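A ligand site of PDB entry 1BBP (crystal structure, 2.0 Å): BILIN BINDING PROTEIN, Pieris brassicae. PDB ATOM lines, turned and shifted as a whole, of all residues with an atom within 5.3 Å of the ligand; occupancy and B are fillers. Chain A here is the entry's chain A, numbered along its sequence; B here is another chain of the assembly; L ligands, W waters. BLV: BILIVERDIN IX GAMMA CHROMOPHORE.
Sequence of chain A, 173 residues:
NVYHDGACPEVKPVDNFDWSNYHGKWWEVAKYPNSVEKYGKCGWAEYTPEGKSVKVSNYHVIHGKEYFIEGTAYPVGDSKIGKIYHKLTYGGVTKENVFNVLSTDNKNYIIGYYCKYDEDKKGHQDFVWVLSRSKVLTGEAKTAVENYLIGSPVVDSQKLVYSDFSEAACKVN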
ATOM      1  N   TRP A  26      -1.729  14.087 -24.849  1.00  0.00           N
ATOM      2  CA  TRP A  26      -2.410  14.817 -23.785  1.00  0.00           C
ATOM      3  C   TRP A  26      -3.776  15.223 -24.313  1.00  0.00           C
ATOM      4  O   TRP A  26      -3.870  15.813 -25.392  1.00  0.00           O
ATOM      5  CB  TRP A  26      -1.576  16.057 -23.450  1.00  0.00           C
ATOM      6  CG  TRP A  26      -0.253  15.645 -22.787  1.00  0.00           C
ATOM      7  CD1 TRP A  26       0.892  15.187 -23.345  1.00  0.00           C
ATOM      8  CD2 TRP A  26      -0.013  15.625 -21.408  1.00  0.00           C
ATOM      9  NE1 TRP A  26       1.838  14.914 -22.344  1.00  0.00           N
ATOM     10  CE2 TRP A  26       1.313  15.184 -21.215  1.00  0.00           C
ATOM     11  CE3 TRP A  26      -0.832  15.953 -20.352  1.00  0.00           C
ATOM     12  CZ2 TRP A  26       1.875  15.088 -19.962  1.00  0.00           C
ATOM     13  CZ3 TRP A  26      -0.270  15.827 -19.091  1.00  0.00           C
ATOM     14  CH2 TRP A  26       1.043  15.414 -18.889  1.00  0.00           C
ATOM     15  N   GLU A  28      -7.151  17.453 -24.292  1.00  0.00           N
ATOM     16  CA  GLU A  28      -7.468  18.750 -23.707  1.00  0.00           C
ATOM     17  C   GLU A  28      -8.802  18.715 -23.008  1.00  0.00           C
ATOM     18  O   GLU A  28      -9.824  18.681 -23.676  1.00  0.00           O
ATOM     19  CB  GLU A  28      -7.274  20.054 -24.523  1.00  0.00           C
ATOM     20  CG  GLU A  28      -8.082  20.079 -25.814  1.00  0.00           C
ATOM     21  CD  GLU A  28      -8.527  21.516 -26.115  1.00  0.00           C
ATOM     22  OE1 GLU A  28      -7.686  22.427 -26.293  1.00  0.00           O
ATOM     23  OE2 GLU A  28      -9.750  21.718 -26.199  1.00  0.00           O
ATOM     24  N   ASN A  34     -11.474  29.865 -27.736  1.00  0.00           N
ATOM     25  CA  ASN A  34     -10.666  30.705 -28.629  1.00  0.00           C
ATOM     26  C   ASN A  34     -11.192  30.526 -30.049  1.00  0.00           C
ATOM     27  O   ASN A  34     -11.861  29.526 -30.310  1.00  0.00           O
ATOM     28  CB  ASN A  34      -9.146  30.404 -28.551  1.00  0.00           C
ATOM     29  CG  ASN A  34      -8.732  28.996 -29.003  1.00  0.00           C
ATOM     30  OD1 ASN A  34      -8.866  28.644 -30.172  1.00  0.00           O
ATOM     31  ND2 ASN A  34      -8.178  28.231 -28.097  1.00  0.00           N
ATOM     32  N   VAL A  36      -9.568  29.908 -32.810  1.00  0.00           N
ATOM     33  CA  VAL A  36      -8.974  28.890 -33.689  1.00  0.00           C
ATOM     34  C   VAL A  36      -9.618  27.520 -33.453  1.00  0.00           C
ATOM     35  O   VAL A  36      -9.788  26.734 -34.385  1.00  0.00           O
ATOM     36  CB  VAL A  36      -7.421  28.817 -33.643  1.00  0.00           C
ATOM     37  CG1 VAL A  36      -6.912  27.663 -32.780  1.00  0.00           C
ATOM     38  CG2 VAL A  36      -6.821  28.673 -35.033  1.00  0.00           C
ATOM     39  N   GLU A  37     -10.050  27.295 -32.220  1.00  0.00           N
ATOM     40  CA  GLU A  37     -10.568  25.995 -31.823  1.00  0.00           C
ATOM     41  C   GLU A  37     -12.081  25.926 -31.837  1.00  0.00           C
ATOM     42  O   GLU A  37     -12.653  24.989 -31.287  1.00  0.00           O
ATOM     43  CB  GLU A  37     -10.036  25.591 -30.439  1.00  0.00           C
ATOM     44  CG  GLU A  37      -8.513  25.446 -30.461  1.00  0.00           C
ATOM     45  CD  GLU A  37      -8.110  24.960 -29.075  1.00  0.00           C
ATOM     46  OE1 GLU A  37      -8.594  23.869 -28.693  1.00  0.00           O
ATOM     47  OE2 GLU A  37      -7.326  25.662 -28.378  1.00  0.00           O
ATOM     48  N   GLY A  43     -10.476  17.215 -28.359  1.00  0.00           N
ATOM     49  CA  GLY A  43      -9.171  17.780 -28.736  1.00  0.00           C
ATOM     50  C   GLY A  43      -8.021  17.077 -28.028  1.00  0.00           C
ATOM     51  O   GLY A  43      -8.146  16.749 -26.852  1.00  0.00           O
ATOM     52  N   TRP A  44      -6.887  17.003 -28.697  1.00  0.00           N
ATOM     53  CA  TRP A  44      -5.655  16.519 -28.041  1.00  0.00           C
ATOM     54  C   TRP A  44      -4.378  17.110 -28.638  1.00  0.00           C
ATOM     55  O   TRP A  44      -4.360  17.635 -29.752  1.00  0.00           O
ATOM     56  CB  TRP A  44      -5.569  14.965 -27.953  1.00  0.00           C
ATOM     57  CG  TRP A  44      -5.185  14.278 -29.278  1.00  0.00           C
ATOM     58  CD1 TRP A  44      -3.950  13.898 -29.694  1.00  0.00           C
ATOM     59  CD2 TRP A  44      -6.045  13.919 -30.316  1.00  0.00           C
ATOM     60  NE1 TRP A  44      -4.033  13.345 -30.990  1.00  0.00           N
ATOM     61  CE2 TRP A  44      -5.263  13.361 -31.350  1.00  0.00           C
ATOM     62  CE3 TRP A  44      -7.414  14.060 -30.442  1.00  0.00           C
ATOM     63  CZ2 TRP A  44      -5.811  12.910 -32.540  1.00  0.00           C
ATOM     64  CZ3 TRP A  44      -7.979  13.602 -31.646  1.00  0.00           C
ATOM     65  CH2 TRP A  44      -7.201  13.045 -32.665  1.00  0.00           C
ATOM     66  N   ALA A  45      -3.339  16.981 -27.878  1.00  0.00           N
ATOM     67  CA  ALA A  45      -1.991  17.377 -28.273  1.00  0.00           C
ATOM     68  C   ALA A  45      -1.099  16.132 -28.286  1.00  0.00           C
ATOM     69  O   ALA A  45      -1.239  15.262 -27.431  1.00  0.00           O
ATOM     70  CB  ALA A  45      -1.431  18.361 -27.234  1.00  0.00           C
ATOM     71  N   TYR A  47       2.893  15.062 -28.315  1.00  0.00           N
ATOM     72  CA  TYR A  47       4.282  15.543 -28.151  1.00  0.00           C
ATOM     73  C   TYR A  47       5.273  14.397 -28.372  1.00  0.00           C
ATOM     74  O   TYR A  47       5.171  13.364 -27.717  1.00  0.00           O
ATOM     75  CB  TYR A  47       4.510  16.175 -26.762  1.00  0.00           C
ATOM     76  CG  TYR A  47       3.536  17.343 -26.498  1.00  0.00           C
ATOM     77  CD1 TYR A  47       3.414  18.379 -27.403  1.00  0.00           C
ATOM     78  CD2 TYR A  47       2.716  17.308 -25.389  1.00  0.00           C
ATOM     79  CE1 TYR A  47       2.495  19.399 -27.192  1.00  0.00           C
ATOM     80  CE2 TYR A  47       1.790  18.307 -25.158  1.00  0.00           C
ATOM     81  CZ  TYR A  47       1.677  19.357 -26.060  1.00  0.00           C
ATOM     82  OH  TYR A  47       0.776  20.366 -25.819  1.00  0.00           O
ATOM     83  N   ASN A  58      -1.325  19.348 -32.692  1.00  0.00           N
ATOM     84  CA  ASN A  58      -2.587  19.582 -31.952  1.00  0.00           C
ATOM     85  C   ASN A  58      -3.758  19.252 -32.845  1.00  0.00           C
ATOM     86  O   ASN A  58      -3.790  19.728 -33.967  1.00  0.00           O
ATOM     87  CB  ASN A  58      -2.668  21.077 -31.619  1.00  0.00           C
ATOM     88  CG  ASN A  58      -1.530  21.395 -30.663  1.00  0.00           C
ATOM     89  OD1 ASN A  58      -0.925  22.472 -30.710  1.00  0.00           O
ATOM     90  ND2 ASN A  58      -1.255  20.439 -29.826  1.00  0.00           N
ATOM     91  N   TYR A  59      -4.649  18.393 -32.385  1.00  0.00           N
ATOM     92  CA  TYR A  59      -5.779  17.929 -33.192  1.00  0.00           C
ATOM     93  C   TYR A  59      -7.092  18.206 -32.486  1.00  0.00           C
ATOM     94  O   TYR A  59      -7.142  18.109 -31.259  1.00  0.00           O
ATOM     95  CB  TYR A  59      -5.789  16.390 -33.325  1.00  0.00           C
ATOM     96  CG  TYR A  59      -4.628  15.826 -34.167  1.00  0.00           C
ATOM     97  CD1 TYR A  59      -4.843  15.505 -35.476  1.00  0.00           C
ATOM     98  CD2 TYR A  59      -3.383  15.631 -33.596  1.00  0.00           C
ATOM     99  CE1 TYR A  59      -3.795  15.020 -36.254  1.00  0.00           C
ATOM    100  CE2 TYR A  59      -2.324  15.142 -34.355  1.00  0.00           C
ATOM    101  CZ  TYR A  59      -2.528  14.862 -35.692  1.00  0.00           C
ATOM    102  OH  TYR A  59      -1.482  14.460 -36.480  1.00  0.00           O
ATOM    103  N   HIS A  60      -8.127  18.211 -33.317  1.00  0.00           N
ATOM    104  CA  HIS A  60      -9.539  18.147 -32.892  1.00  0.00           C
ATOM    105  C   HIS A  60     -10.441  17.680 -34.017  1.00  0.00           C
ATOM    106  O   HIS A  60     -10.015  17.607 -35.178  1.00  0.00           O
ATOM    107  CB  HIS A  60     -10.095  19.434 -32.216  1.00  0.00           C
ATOM    108  CG  HIS A  60     -10.311  20.685 -33.114  1.00  0.00           C
ATOM    109  ND1 HIS A  60     -10.303  21.986 -32.543  1.00  0.00           N
ATOM    110  CD2 HIS A  60     -10.580  20.798 -34.438  1.00  0.00           C
ATOM    111  CE1 HIS A  60     -10.573  22.905 -33.586  1.00  0.00           C
ATOM    112  NE2 HIS A  60     -10.748  22.170 -34.768  1.00  0.00           N
ATOM    113  N   TYR A  67      -8.803  18.043 -37.934  1.00  0.00           N
ATOM    114  CA  TYR A  67      -8.074  19.303 -38.168  1.00  0.00           C
ATOM    115  C   TYR A  67      -6.872  19.322 -37.227  1.00  0.00           C
ATOM    116  O   TYR A  67      -6.978  18.913 -36.071  1.00  0.00           O
ATOM    117  CB  TYR A  67      -8.939  20.532 -37.778  1.00  0.00           C
ATOM    118  CG  TYR A  67     -10.153  20.690 -38.704  1.00  0.00           C
ATOM    119  CD1 TYR A  67     -11.357  20.081 -38.418  1.00  0.00           C
ATOM    120  CD2 TYR A  67     -10.024  21.433 -39.859  1.00  0.00           C
ATOM    121  CE1 TYR A  67     -12.437  20.216 -39.275  1.00  0.00           C
ATOM    122  CE2 TYR A  67     -11.099  21.580 -40.722  1.00  0.00           C
ATOM    123  CZ  TYR A  67     -12.307  20.972 -40.423  1.00  0.00           C
ATOM    124  OH  TYR A  67     -13.386  21.164 -41.250  1.00  0.00           O
ATOM    125  N   PHE A  68      -5.768  19.855 -37.696  1.00  0.00           N
ATOM    126  CA  PHE A  68      -4.617  19.945 -36.819  1.00  0.00           C
ATOM    127  C   PHE A  68      -3.679  21.082 -37.195  1.00  0.00           C
ATOM    128  O   PHE A  68      -3.720  21.542 -38.342  1.00  0.00           O
ATOM    129  CB  PHE A  68      -3.871  18.583 -36.813  1.00  0.00           C
ATOM    130  CG  PHE A  68      -3.259  18.204 -38.179  1.00  0.00           C
ATOM    131  CD1 PHE A  68      -4.042  17.625 -39.148  1.00  0.00           C
ATOM    132  CD2 PHE A  68      -1.928  18.478 -38.420  1.00  0.00           C
ATOM    133  CE1 PHE A  68      -3.499  17.325 -40.390  1.00  0.00           C
ATOM    134  CE2 PHE A  68      -1.385  18.189 -39.655  1.00  0.00           C
ATOM    135  CZ  PHE A  68      -2.170  17.617 -40.647  1.00  0.00           C
ATOM    136  N   ILE A  69      -2.749  21.359 -36.302  1.00  0.00           N
ATOM    137  CA  ILE A  69      -1.573  22.214 -36.573  1.00  0.00           C
ATOM    138  C   ILE A  69      -0.323  21.434 -36.129  1.00  0.00           C
ATOM    139  O   ILE A  69      -0.377  20.715 -35.128  1.00  0.00           O
ATOM    140  CB  ILE A  69      -1.685  23.521 -35.744  1.00  0.00           C
ATOM    141  CG1 ILE A  69      -0.527  24.543 -35.906  1.00  0.00           C
ATOM    142  CG2 ILE A  69      -1.855  23.211 -34.246  1.00  0.00           C
ATOM    143  CD1 ILE A  69      -0.774  25.615 -36.967  1.00  0.00           C
ATOM    144  N   HIS A  86       6.273  27.560 -27.817  1.00  0.00           N
ATOM    145  CA  HIS A  86       5.603  26.738 -28.817  1.00  0.00           C
ATOM    146  C   HIS A  86       5.570  27.530 -30.104  1.00  0.00           C
ATOM    147  O   HIS A  86       4.984  28.614 -30.108  1.00  0.00           O
ATOM    148  CB  HIS A  86       4.156  26.420 -28.397  1.00  0.00           C
ATOM    149  CG  HIS A  86       4.178  25.470 -27.402  1.00  0.00           C
ATOM    150  ND1 HIS A  86       3.526  24.297 -27.578  1.00  0.00           N
ATOM    151  CD2 HIS A  86       4.786  25.572 -26.280  1.00  0.00           C
ATOM    152  CE1 HIS A  86       3.761  23.645 -26.501  1.00  0.00           C
ATOM    153  NE2 HIS A  86       4.520  24.384 -25.701  1.00  0.00           N
ATOM    154  N   LEU A  88       4.714  28.166 -33.635  1.00  0.00           N
ATOM    155  CA  LEU A  88       3.601  27.829 -34.552  1.00  0.00           C
ATOM    156  C   LEU A  88       3.498  28.950 -35.579  1.00  0.00           C
ATOM    157  O   LEU A  88       3.922  30.076 -35.309  1.00  0.00           O
ATOM    158  CB  LEU A  88       2.245  27.762 -33.800  1.00  0.00           C
ATOM    159  CG  LEU A  88       2.212  26.719 -32.664  1.00  0.00           C
ATOM    160  CD1 LEU A  88       1.115  26.992 -31.614  1.00  0.00           C
ATOM    161  CD2 LEU A  88       2.149  25.278 -33.206  1.00  0.00           C
ATOM    162  N   TYR A  90       0.779  31.200 -37.450  1.00  0.00           N
ATOM    163  CA  TYR A  90      -0.590  31.626 -37.733  1.00  0.00           C
ATOM    164  C   TYR A  90      -0.605  32.814 -38.694  1.00  0.00           C
ATOM    165  O   TYR A  90       0.025  33.834 -38.432  1.00  0.00           O
ATOM    166  CB  TYR A  90      -1.366  31.975 -36.453  1.00  0.00           C
ATOM    167  CG  TYR A  90      -1.727  30.725 -35.643  1.00  0.00           C
ATOM    168  CD1 TYR A  90      -0.937  30.338 -34.574  1.00  0.00           C
ATOM    169  CD2 TYR A  90      -2.846  29.987 -35.984  1.00  0.00           C
ATOM    170  CE1 TYR A  90      -1.284  29.212 -33.815  1.00  0.00           C
ATOM    171  CE2 TYR A  90      -3.204  28.877 -35.236  1.00  0.00           C
ATOM    172  CZ  TYR A  90      -2.432  28.489 -34.136  1.00  0.00           C
ATOM    173  OH  TYR A  90      -2.799  27.411 -33.370  1.00  0.00           O
ATOM    174  N   ASN A  97       5.641  31.352 -29.113  1.00  0.00           N
ATOM    175  CA  ASN A  97       4.589  31.657 -28.160  1.00  0.00           C
ATOM    176  C   ASN A  97       4.913  31.015 -26.820  1.00  0.00           C
ATOM    177  O   ASN A  97       5.283  29.844 -26.807  1.00  0.00           O
ATOM    178  CB  ASN A  97       3.301  31.064 -28.690  1.00  0.00           C
ATOM    179  CG  ASN A  97       3.004  31.601 -30.093  1.00  0.00           C
ATOM    180  OD1 ASN A  97       3.013  30.855 -31.061  1.00  0.00           O
ATOM    181  ND2 ASN A  97       2.733  32.888 -30.262  1.00  0.00           N
ATOM    182  N   VAL A  98       4.964  31.831 -25.774  1.00  0.00           N
ATOM    183  CA  VAL A  98       5.300  31.363 -24.419  1.00  0.00           C
ATOM    184  C   VAL A  98       4.065  30.760 -23.770  1.00  0.00           C
ATOM    185  O   VAL A  98       3.151  31.482 -23.355  1.00  0.00           O
ATOM    186  CB  VAL A  98       5.822  32.496 -23.515  1.00  0.00           C
ATOM    187  CG1 VAL A  98       6.017  32.052 -22.045  1.00  0.00           C
ATOM    188  CG2 VAL A  98       7.116  33.108 -24.069  1.00  0.00           C
ATOM    189  N   PHE A  99       4.186  29.461 -23.585  1.00  0.00           N
ATOM    190  CA  PHE A  99       3.257  28.689 -22.781  1.00  0.00           C
ATOM    191  C   PHE A  99       3.833  28.586 -21.374  1.00  0.00           C
ATOM    192  O   PHE A  99       5.040  28.379 -21.213  1.00  0.00           O
ATOM    193  CB  PHE A  99       3.179  27.322 -23.450  1.00  0.00           C
ATOM    194  CG  PHE A  99       2.284  26.286 -22.725  1.00  0.00           C
ATOM    195  CD1 PHE A  99       0.910  26.352 -22.851  1.00  0.00           C
ATOM    196  CD2 PHE A  99       2.871  25.253 -22.011  1.00  0.00           C
ATOM    197  CE1 PHE A  99       0.118  25.373 -22.257  1.00  0.00           C
ATOM    198  CE2 PHE A  99       2.090  24.267 -21.420  1.00  0.00           C
ATOM    199  CZ  PHE A  99       0.708  24.330 -21.542  1.00  0.00           C
ATOM    200  N   TYR A 114      -1.261  30.920 -21.989  1.00  0.00           N
ATOM    201  CA  TYR A 114      -0.651  31.822 -22.989  1.00  0.00           C
ATOM    202  C   TYR A 114      -1.449  33.124 -23.079  1.00  0.00           C
ATOM    203  O   TYR A 114      -2.678  33.114 -23.161  1.00  0.00           O
ATOM    204  CB  TYR A 114      -0.628  31.091 -24.364  1.00  0.00           C
ATOM    205  CG  TYR A 114      -0.448  32.032 -25.574  1.00  0.00           C
ATOM    206  CD1 TYR A 114       0.709  32.769 -25.737  1.00  0.00           C
ATOM    207  CD2 TYR A 114      -1.472  32.134 -26.493  1.00  0.00           C
ATOM    208  CE1 TYR A 114       0.811  33.632 -26.799  1.00  0.00           C
ATOM    209  CE2 TYR A 114      -1.368  33.007 -27.570  1.00  0.00           C
ATOM    210  CZ  TYR A 114      -0.235  33.761 -27.704  1.00  0.00           C
ATOM    211  OH  TYR A 114      -0.131  34.605 -28.751  1.00  0.00           O
ATOM    212  N   LYS A 116      -1.970  36.580 -25.354  1.00  0.00           N
ATOM    213  CA  LYS A 116      -1.768  37.313 -26.597  1.00  0.00           C
ATOM    214  C   LYS A 116      -2.020  38.780 -26.314  1.00  0.00           C
ATOM    215  O   LYS A 116      -3.137  39.126 -25.954  1.00  0.00           O
ATOM    216  CB  LYS A 116      -2.824  36.877 -27.604  1.00  0.00           C
ATOM    217  CG  LYS A 116      -2.578  37.458 -28.984  1.00  0.00           C
ATOM    218  CD  LYS A 116      -3.630  36.905 -29.928  1.00  0.00           C
ATOM    219  CE  LYS A 116      -3.500  37.498 -31.349  1.00  0.00           C
ATOM    220  NZ  LYS A 116      -4.644  37.005 -32.175  1.00  0.00           N
ATOM    221  N   PHE A 127      -5.463  32.683 -22.948  1.00  0.00           N
ATOM    222  CA  PHE A 127      -5.662  31.306 -23.412  1.00  0.00           C
ATOM    223  C   PHE A 127      -5.179  30.352 -22.331  1.00  0.00           C
ATOM    224  O   PHE A 127      -4.057  30.507 -21.856  1.00  0.00           O
ATOM    225  CB  PHE A 127      -4.874  30.956 -24.560  1.00  0.00           C
ATOM    226  CG  PHE A 127      -5.144  31.746 -25.795  1.00  0.00           C
ATOM    227  CD1 PHE A 127      -4.970  33.128 -25.797  1.00  0.00           C
ATOM    228  CD2 PHE A 127      -5.547  31.052 -26.929  1.00  0.00           C
ATOM    229  CE1 PHE A 127      -5.199  33.832 -26.971  1.00  0.00           C
ATOM    230  CE2 PHE A 127      -5.780  31.753 -28.112  1.00  0.00           C
ATOM    231  CZ  PHE A 127      -5.607  33.154 -28.130  1.00  0.00           C
ATOM    232  N   TRP A 129      -5.429  26.079 -21.023  1.00  0.00           N
ATOM    233  CA  TRP A 129      -5.707  24.673 -21.363  1.00  0.00           C
ATOM    234  C   TRP A 129      -5.450  23.851 -20.102  1.00  0.00           C
ATOM    235  O   TRP A 129      -4.380  24.026 -19.518  1.00  0.00           O
ATOM    236  CB  TRP A 129      -4.756  24.126 -22.465  1.00  0.00           C
ATOM    237  CG  TRP A 129      -4.972  24.799 -23.829  1.00  0.00           C
ATOM    238  CD1 TRP A 129      -5.895  24.510 -24.756  1.00  0.00           C
ATOM    239  CD2 TRP A 129      -4.267  25.911 -24.329  1.00  0.00           C
ATOM    240  NE1 TRP A 129      -5.776  25.441 -25.822  1.00  0.00           N
ATOM    241  CE2 TRP A 129      -4.818  26.245 -25.561  1.00  0.00           C
ATOM    242  CE3 TRP A 129      -3.211  26.635 -23.785  1.00  0.00           C
ATOM    243  CZ2 TRP A 129      -4.361  27.322 -26.311  1.00  0.00           C
ATOM    244  CZ3 TRP A 129      -2.753  27.724 -24.528  1.00  0.00           C
ATOM    245  CH2 TRP A 129      -3.311  28.065 -25.770  1.00  0.00           C
ATOM    246  N   LEU A 131      -4.660  20.075 -19.710  1.00  0.00           N
ATOM    247  CA  LEU A 131      -4.226  18.923 -20.513  1.00  0.00           C
ATOM    248  C   LEU A 131      -3.976  17.777 -19.546  1.00  0.00           C
ATOM    249  O   LEU A 131      -3.505  18.035 -18.438  1.00  0.00           O
ATOM    250  CB  LEU A 131      -2.888  19.204 -21.201  1.00  0.00           C
ATOM    251  CG  LEU A 131      -2.945  20.454 -22.081  1.00  0.00           C
ATOM    252  CD1 LEU A 131      -1.528  20.965 -22.403  1.00  0.00           C
ATOM    253  CD2 LEU A 131      -3.809  20.224 -23.333  1.00  0.00           C
ATOM    254  N   LYS B 121     -18.088  24.377 -40.823  1.00  0.00           N
ATOM    255  CA  LYS B 121     -17.950  23.714 -39.517  1.00  0.00           C
ATOM    256  C   LYS B 121     -19.275  23.312 -38.903  1.00  0.00           C
ATOM    257  O   LYS B 121     -19.258  22.810 -37.778  1.00  0.00           O
ATOM    258  CB  LYS B 121     -17.121  24.595 -38.606  1.00  0.00           C
ATOM    259  CG  LYS B 121     -15.787  24.952 -39.267  1.00  0.00           C
ATOM    260  CD  LYS B 121     -14.713  25.432 -38.292  1.00  0.00           C
ATOM    261  CE  LYS B 121     -13.368  25.661 -38.992  1.00  0.00           C
ATOM    262  NZ  LYS B 121     -12.414  26.392 -38.154  1.00  0.00           N
HETATM  263  NA  BLV L   1      -4.847  24.619 -32.944  1.00  0.00           N
HETATM  264  C1A BLV L   1      -4.861  24.802 -34.255  1.00  0.00           C
HETATM  265  C2A BLV L   1      -5.733  23.797 -34.886  1.00  0.00           C
HETATM  266  C3A BLV L   1      -6.223  23.023 -33.840  1.00  0.00           C
HETATM  267  C4A BLV L   1      -5.647  23.534 -32.657  1.00  0.00           C
HETATM  268  CMA BLV L   1      -7.111  21.858 -33.956  1.00  0.00           C
HETATM  269  OA  BLV L   1      -4.198  25.621 -34.883  1.00  0.00           O
HETATM  270  CAA BLV L   1      -6.087  23.713 -36.310  1.00  0.00           C
HETATM  271  CBA BLV L   1      -7.281  24.649 -36.573  1.00  0.00           C
HETATM  272  CGA BLV L   1      -7.641  24.567 -38.051  1.00  0.00           C
HETATM  273  O1A BLV L   1      -6.707  24.483 -38.886  1.00  0.00           O
HETATM  274  O2A BLV L   1      -8.855  24.593 -38.375  1.00  0.00           O
HETATM  275  CHB BLV L   1      -5.956  23.014 -31.389  1.00  0.00           C
HETATM  276  NB  BLV L   1      -4.263  23.956 -29.791  1.00  0.00           N
HETATM  277  C1B BLV L   1      -5.202  23.009 -30.215  1.00  0.00           C
HETATM  278  C2B BLV L   1      -5.424  22.061 -29.199  1.00  0.00           C
HETATM  279  C3B BLV L   1      -4.528  22.379 -28.154  1.00  0.00           C
HETATM  280  C4B BLV L   1      -3.852  23.562 -28.524  1.00  0.00           C
HETATM  281  CMB BLV L   1      -6.426  20.966 -29.236  1.00  0.00           C
HETATM  282  CAB BLV L   1      -4.363  21.737 -26.832  1.00  0.00           C
HETATM  283  CBB BLV L   1      -4.258  20.207 -26.850  1.00  0.00           C
HETATM  284  CHC BLV L   1      -2.962  24.184 -27.639  1.00  0.00           C
HETATM  285  NC  BLV L   1      -2.054  26.183 -28.778  1.00  0.00           N
HETATM  286  C1C BLV L   1      -2.064  25.243 -27.794  1.00  0.00           C
HETATM  287  C2C BLV L   1      -1.021  25.492 -26.899  1.00  0.00           C
HETATM  288  C3C BLV L   1      -0.386  26.713 -27.284  1.00  0.00           C
HETATM  289  C4C BLV L   1      -1.051  27.100 -28.489  1.00  0.00           C
HETATM  290  CMC BLV L   1      -0.670  24.631 -25.762  1.00  0.00           C
HETATM  291  CAC BLV L   1       0.710  27.362 -26.523  1.00  0.00           C
HETATM  292  CBC BLV L   1       1.242  28.722 -26.976  1.00  0.00           C
HETATM  293  CHD BLV L   1      -0.880  28.271 -29.214  1.00  0.00           C
HETATM  294  ND  BLV L   1      -3.256  28.594 -29.925  1.00  0.00           N
HETATM  295  C1D BLV L   1      -1.920  29.001 -29.808  1.00  0.00           C
HETATM  296  C2D BLV L   1      -1.754  30.252 -30.394  1.00  0.00           C
HETATM  297  C3D BLV L   1      -3.003  30.581 -30.977  1.00  0.00           C
HETATM  298  C4D BLV L   1      -3.931  29.503 -30.577  1.00  0.00           C
HETATM  299  CMD BLV L   1      -0.481  30.991 -30.486  1.00  0.00           C
HETATM  300  OD  BLV L   1      -5.129  29.432 -30.871  1.00  0.00           O
HETATM  301  CAD BLV L   1      -3.303  31.613 -31.981  1.00  0.00           C
HETATM  302  CBD BLV L   1      -3.609  32.950 -31.355  1.00  0.00           C
HETATM  303  CGD BLV L   1      -3.973  33.786 -32.571  1.00  0.00           C
HETATM  304  O1D BLV L   1      -3.041  34.280 -33.255  1.00  0.00           O
HETATM  305  O2D BLV L   1      -5.193  33.912 -32.840  1.00  0.00           O
HETATM  306  O   HOH W   1      -5.275  26.656 -30.220  1.00  0.00           O
HETATM  307  O   HOH W   2       0.283  33.709 -32.321  1.00  0.00           O
HETATM  308  O   HOH W   3      -7.402  33.891 -34.406  1.00  0.00           O
HETATM  309  O   HOH W   4      -7.326  31.732 -31.567  1.00  0.00           O
HETATM  310  O   HOH W   5     -11.076  23.876 -36.995  1.00  0.00           O
HETATM  311  O   HOH W   6      -2.537  25.364 -31.404  1.00  0.00           O
HETATM  312  O   HOH W   7       1.077  24.019 -29.169  1.00  0.00           O
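The side-chain hydroxyl of Tyr 90 sits at hydrogen-bond distance from an oxygen (OA) of the ligand (2.7 Å).
NZ of Lys 121 of chain B is in salt-bridge range of O2A of the ligand.
O2D of the ligand is in salt-bridge range of NZ of Lys 116, at 3.2 Å.
The backbone NH of Phe 127 is in hydrogen-bond range of the backbone carbonyl oxygen of Tyr 114 (2.8 Å).
N of Val 36 is in hydrogen-bond range of OD1 of Asn 34.
The indole nitrogen of Trp 129 sits at hydrogen-bond distance from the side-chain carboxylate of Glu 37 (3.0 Å).
O of Ile 69 sits at hydrogen-bond distance from N of Asn 58 (2.9 Å).
The backbone carbonyl oxygen (O) of His 60 is in hydrogen-bond range of the backbone NH (N) of Tyr 67, 3.0 Å away.
N of Glu 28 sits at hydrogen-bond distance from O of Gly 43 (2.8 Å).
The backbone carbonyl oxygen of Asn 97 is in hydrogen-bond range of the backbone NH of His 86, 2.7 Å away.
The backbone NH (N) of Tyr 59 is in hydrogen-bond range of the backbone carbonyl oxygen (O) of Trp 44 (2.8 Å).
OE1 of Glu 28 touches CAB of the ligand, 3.4 Å away.
Asn 34 touches the ligand.
Val 36 touches the ligand.
Glu 37 touches the ligand.
Trp 44 touches the ligand (C to CBB, 3.6 Å).
Ala 45 touches the ligand.
Asn 58 touches the ligand.
O of Tyr 59 touches CMB of the ligand (3.6 Å).
ND1 of His 60 touches CMA of the ligand (3.5 Å).
Tyr 67 touches the ligand.
Phe 68 touches the ligand (C to CAA, 3.7 Å).
Ile 69 touches the ligand.
CB of His 86 touches CBC of the ligand (3.98 Å).
Leu 88 touches the ligand.
Asn 97 touches the ligand.
CE1 of Phe 99 touches CMC of the ligand (3.7 Å).
Tyr 114 touches the ligand (CE2 to CMD, 3.7 Å).
CE2 of Phe 127 touches OD of the ligand (3.7 Å).
Trp 129 touches the ligand (CZ2 to C1C, 3.4 Å).
Leu 131 touches the ligand.
Hydrophobic or aromatic side chains that line the ligand: Val 36, Ala 45, His 60, Tyr 67, Ile 69, His 86, Leu 88, Tyr 90, Phe 99, Tyr 114, Phe 127, Trp 129 and Leu 131.
Of the 27 residues printed, 23 come within 4 Å of the ligand.
The nearest printed residue that does not touch the ligand is Gly 43 (4.2 Å).
Water W5 lies within hydrogen-bond range of O2A of the ligand (2.7 Å), NE2 of His 60 (2.8 Å) and NZ of Lys 121 of chain B (3.1 Å).
Water W6 lies within hydrogen-bond range of NB of the ligand (2.8 Å), OH of Tyr 90 (2.9 Å) and OD1 of Asn 58 (3.4 Å).
Water W1 lies within hydrogen-bond range of a nitrogen (ND) of the ligand (2.8 Å) and the side-chain carboxylate (OE2) of Glu 37 (2.9 Å).
Water W4 lies within hydrogen-bond range of the backbone NH of Val 36 (3.1 Å) and an oxygen (OD) of the ligand (3.3 Å).
Water W7 lies within hydrogen-bond range of a ring nitrogen (ND1) of His 86 and the side-chain amide oxygen of Asn 58.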
